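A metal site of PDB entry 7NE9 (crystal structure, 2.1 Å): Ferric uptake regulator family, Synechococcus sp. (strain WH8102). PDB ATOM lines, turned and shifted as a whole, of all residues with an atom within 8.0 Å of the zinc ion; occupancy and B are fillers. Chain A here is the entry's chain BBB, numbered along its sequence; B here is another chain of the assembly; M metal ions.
The zinc ion is bound by the side-chain sulfur (SG) of Cys 86 (2.3 Å), the side-chain sulfur (SG) of Cys 123 (2.3 Å), the side-chain sulfur (SG) of Cys 126 (2.3 Å) and the side-chain sulfur (SG) of Cys 83 (2.4 Å).
The zinc ion has four donor atoms within binding distance.
Four residues have an atom within 4 Å of the zinc ion: Cys 83, Cys 86, Cys 123 and Cys 126.
The side-chain sulfur (SG) of Cys 86 lies close to the backbone NH (N) of Thr 88, 3.5 Å away.
SG of Cys 123 sits close to N of Ser 125 (3.7 Å).
The side-chain sulfur (SG) of Cys 126 lies close to the side-chain carboxylate (OD2) of Asp 85, 3.7 Å away.
The backbone NH (N) of Cys 83 sits at hydrogen-bond distance from the backbone carbonyl oxygen (O) of Thr 88 (2.9 Å).
The side-chain sulfur (SG) of Cys 83 lies close to the backbone NH (N) of Asp 85 (3.4 Å).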
ATOM      1  N   THR A  82     -22.849 -17.329 -20.631  1.00  0.00           N
ATOM      2  CA  THR A  82     -23.052 -16.836 -21.999  1.00  0.00           C
ATOM      3  C   THR A  82     -24.481 -16.286 -22.111  1.00  0.00           C
ATOM      4  O   THR A  82     -25.413 -16.975 -21.686  1.00  0.00           O
ATOM      5  CB  THR A  82     -22.759 -17.943 -23.025  1.00  0.00           C
ATOM      6  OG1 THR A  82     -21.418 -18.384 -22.831  1.00  0.00           O
ATOM      7  CG2 THR A  82     -22.941 -17.472 -24.443  1.00  0.00           C
ATOM      8  N   CYS A  83     -24.626 -15.094 -22.669  1.00  0.00           N
ATOM      9  CA  CYS A  83     -25.937 -14.506 -23.023  1.00  0.00           C
ATOM     10  C   CYS A  83     -26.482 -15.202 -24.273  1.00  0.00           C
ATOM     11  O   CYS A  83     -25.784 -15.220 -25.297  1.00  0.00           O
ATOM     12  CB  CYS A  83     -25.849 -13.003 -23.233  1.00  0.00           C
ATOM     13  SG  CYS A  83     -27.464 -12.258 -23.628  1.00  0.00           S
ATOM     14  N   VAL A  84     -27.694 -15.741 -24.205  1.00  0.00           N
ATOM     15  CA  VAL A  84     -28.327 -16.483 -25.332  1.00  0.00           C
ATOM     16  C   VAL A  84     -28.751 -15.487 -26.428  1.00  0.00           C
ATOM     17  O   VAL A  84     -29.012 -15.928 -27.555  1.00  0.00           O
ATOM     18  CB  VAL A  84     -29.523 -17.330 -24.859  1.00  0.00           C
ATOM     19  CG1 VAL A  84     -29.128 -18.338 -23.807  1.00  0.00           C
ATOM     20  CG2 VAL A  84     -30.667 -16.485 -24.335  1.00  0.00           C
ATOM     21  N   ASP A  85     -28.878 -14.199 -26.100  1.00  0.00           N
ATOM     22  CA  ASP A  85     -29.290 -13.161 -27.073  1.00  0.00           C
ATOM     23  C   ASP A  85     -28.043 -12.678 -27.846  1.00  0.00           C
ATOM     24  O   ASP A  85     -27.944 -12.995 -29.050  1.00  0.00           O
ATOM     25  CB  ASP A  85     -30.064 -12.038 -26.396  1.00  0.00           C
ATOM     26  CG  ASP A  85     -30.784 -11.127 -27.395  1.00  0.00           C
ATOM     27  OD1 ASP A  85     -30.576 -11.316 -28.610  1.00  0.00           O
ATOM     28  OD2 ASP A  85     -31.548 -10.242 -26.960  1.00  0.00           O
ATOM     29  N   CYS A  86     -27.130 -11.960 -27.194  1.00  0.00           N
ATOM     30  CA  CYS A  86     -25.975 -11.286 -27.845  1.00  0.00           C
ATOM     31  C   CYS A  86     -24.713 -12.177 -27.894  1.00  0.00           C
ATOM     32  O   CYS A  86     -23.778 -11.797 -28.594  1.00  0.00           O
ATOM     33  CB  CYS A  86     -25.679  -9.971 -27.148  1.00  0.00           C
ATOM     34  SG  CYS A  86     -24.949 -10.141 -25.488  1.00  0.00           S
ATOM     35  N   GLY A  87     -24.674 -13.306 -27.187  1.00  0.00           N
ATOM     36  CA  GLY A  87     -23.499 -14.215 -27.205  1.00  0.00           C
ATOM     37  C   GLY A  87     -22.342 -13.720 -26.348  1.00  0.00           C
ATOM     38  O   GLY A  87     -21.317 -14.361 -26.338  1.00  0.00           O
ATOM     39  N   THR A  88     -22.475 -12.606 -25.614  1.00  0.00           N
ATOM     40  CA  THR A  88     -21.389 -12.152 -24.701  1.00  0.00           C
ATOM     41  C   THR A  88     -21.133 -13.250 -23.643  1.00  0.00           C
ATOM     42  O   THR A  88     -22.095 -13.898 -23.212  1.00  0.00           O
ATOM     43  CB  THR A  88     -21.705 -10.786 -24.067  1.00  0.00           C
ATOM     44  OG1 THR A  88     -20.494 -10.346 -23.477  1.00  0.00           O
ATOM     45  CG2 THR A  88     -22.769 -10.806 -22.988  1.00  0.00           C
ATOM     46  N   THR A  89     -19.866 -13.477 -23.283  1.00  0.00           N
ATOM     47  CA  THR A  89     -19.411 -14.672 -22.528  1.00  0.00           C
ATOM     48  C   THR A  89     -18.357 -14.225 -21.513  1.00  0.00           C
ATOM     49  O   THR A  89     -17.572 -13.374 -21.840  1.00  0.00           O
ATOM     50  CB  THR A  89     -18.905 -15.802 -23.449  1.00  0.00           C
ATOM     51  OG1 THR A  89     -18.800 -16.999 -22.663  1.00  0.00           O
ATOM     52  CG2 THR A  89     -17.605 -15.498 -24.163  1.00  0.00           C
ATOM     53  N   GLY A 121     -27.949 -17.510 -20.069  1.00  0.00           N
ATOM     54  CA  GLY A 121     -28.963 -16.588 -19.557  1.00  0.00           C
ATOM     55  C   GLY A 121     -29.016 -15.316 -20.384  1.00  0.00           C
ATOM     56  O   GLY A 121     -28.631 -15.351 -21.568  1.00  0.00           O
ATOM     57  N   PHE A 122     -29.512 -14.243 -19.806  1.00  0.00           N
ATOM     58  CA  PHE A 122     -29.589 -12.898 -20.427  1.00  0.00           C
ATOM     59  C   PHE A 122     -28.659 -11.967 -19.677  1.00  0.00           C
ATOM     60  O   PHE A 122     -28.771 -11.903 -18.445  1.00  0.00           O
ATOM     61  CB  PHE A 122     -31.007 -12.333 -20.367  1.00  0.00           C
ATOM     62  CG  PHE A 122     -32.061 -13.156 -21.072  1.00  0.00           C
ATOM     63  CD1 PHE A 122     -32.014 -13.331 -22.441  1.00  0.00           C
ATOM     64  CD2 PHE A 122     -33.137 -13.688 -20.368  1.00  0.00           C
ATOM     65  CE1 PHE A 122     -32.997 -14.072 -23.085  1.00  0.00           C
ATOM     66  CE2 PHE A 122     -34.132 -14.400 -21.018  1.00  0.00           C
ATOM     67  CZ  PHE A 122     -34.051 -14.602 -22.376  1.00  0.00           C
ATOM     68  N   CYS A 123     -27.781 -11.263 -20.392  1.00  0.00           N
ATOM     69  CA  CYS A 123     -26.968 -10.159 -19.825  1.00  0.00           C
ATOM     70  C   CYS A 123     -27.864  -8.947 -19.539  1.00  0.00           C
ATOM     71  O   CYS A 123     -29.032  -8.953 -19.980  1.00  0.00           O
ATOM     72  CB  CYS A 123     -25.810  -9.837 -20.760  1.00  0.00           C
ATOM     73  SG  CYS A 123     -26.304  -8.817 -22.186  1.00  0.00           S
ATOM     74  N   SER A 124     -27.339  -7.957 -18.828  1.00  0.00           N
ATOM     75  CA  SER A 124     -28.020  -6.690 -18.416  1.00  0.00           C
ATOM     76  C   SER A 124     -28.712  -6.036 -19.613  1.00  0.00           C
ATOM     77  O   SER A 124     -29.892  -5.667 -19.481  1.00  0.00           O
ATOM     78  CB  SER A 124     -27.049  -5.712 -17.771  1.00  0.00           C
ATOM     79  OG  SER A 124     -26.429  -6.270 -16.628  1.00  0.00           O
ATOM     80  N   SER A 125     -28.003  -5.861 -20.733  1.00  0.00           N
ATOM     81  CA  SER A 125     -28.520  -5.217 -21.970  1.00  0.00           C
ATOM     82  C   SER A 125     -29.733  -5.972 -22.538  1.00  0.00           C
ATOM     83  O   SER A 125     -30.622  -5.306 -23.083  1.00  0.00           O
ATOM     84  CB  SER A 125     -27.461  -5.107 -23.019  1.00  0.00           C
ATOM     85  OG  SER A 125     -26.245  -4.662 -22.453  1.00  0.00           O
ATOM     86  N   CYS A 126     -29.764  -7.308 -22.456  1.00  0.00           N
ATOM     87  CA  CYS A 126     -30.708  -8.162 -23.225  1.00  0.00           C
ATOM     88  C   CYS A 126     -31.919  -8.599 -22.365  1.00  0.00           C
ATOM     89  O   CYS A 126     -32.879  -9.152 -22.927  1.00  0.00           O
ATOM     90  CB  CYS A 126     -29.969  -9.386 -23.763  1.00  0.00           C
ATOM     91  SG  CYS A 126     -28.651  -9.058 -24.991  1.00  0.00           S
ATOM     92  N   ARG A 127     -31.862  -8.459 -21.036  1.00  0.00           N
ATOM     93  CA  ARG A 127     -32.863  -9.038 -20.091  1.00  0.00           C
ATOM     94  C   ARG A 127     -34.226  -8.360 -20.282  1.00  0.00           C
ATOM     95  O   ARG A 127     -34.318  -7.142 -20.152  1.00  0.00           O
ATOM     96  CB  ARG A 127     -32.377  -8.935 -18.640  1.00  0.00           C
ATOM     97  CG  ARG A 127     -33.245  -9.613 -17.588  1.00  0.00           C
ATOM     98  CD  ARG A 127     -33.252  -8.913 -16.241  1.00  0.00           C
ATOM     99  NE  ARG A 127     -32.093  -9.255 -15.421  1.00  0.00           N
ATOM    100  CZ  ARG A 127     -32.107 -10.026 -14.318  1.00  0.00           C
ATOM    101  NH1 ARG A 127     -33.218 -10.583 -13.864  1.00  0.00           N
ATOM    102  NH2 ARG A 127     -30.970 -10.258 -13.671  1.00  0.00           N
ATOM    103  N   PHE B 110     -27.071 -10.557 -14.099  1.00  0.00           N
ATOM    104  CA  PHE B 110     -27.178 -11.599 -15.144  1.00  0.00           C
ATOM    105  C   PHE B 110     -28.320 -12.572 -14.773  1.00  0.00           C
ATOM    106  O   PHE B 110     -28.315 -13.059 -13.655  1.00  0.00           O
ATOM    107  CB  PHE B 110     -25.831 -12.308 -15.268  1.00  0.00           C
ATOM    108  CG  PHE B 110     -25.743 -13.281 -16.410  1.00  0.00           C
ATOM    109  CD1 PHE B 110     -25.369 -12.832 -17.679  1.00  0.00           C
ATOM    110  CD2 PHE B 110     -26.053 -14.619 -16.236  1.00  0.00           C
ATOM    111  CE1 PHE B 110     -25.310 -13.715 -18.745  1.00  0.00           C
ATOM    112  CE2 PHE B 110     -25.995 -15.505 -17.311  1.00  0.00           C
ATOM    113  CZ  PHE B 110     -25.628 -15.041 -18.563  1.00  0.00           C
HETATM  114 ZN    ZN M   1     -26.748 -10.058 -24.085  1.00  0.00          ZN
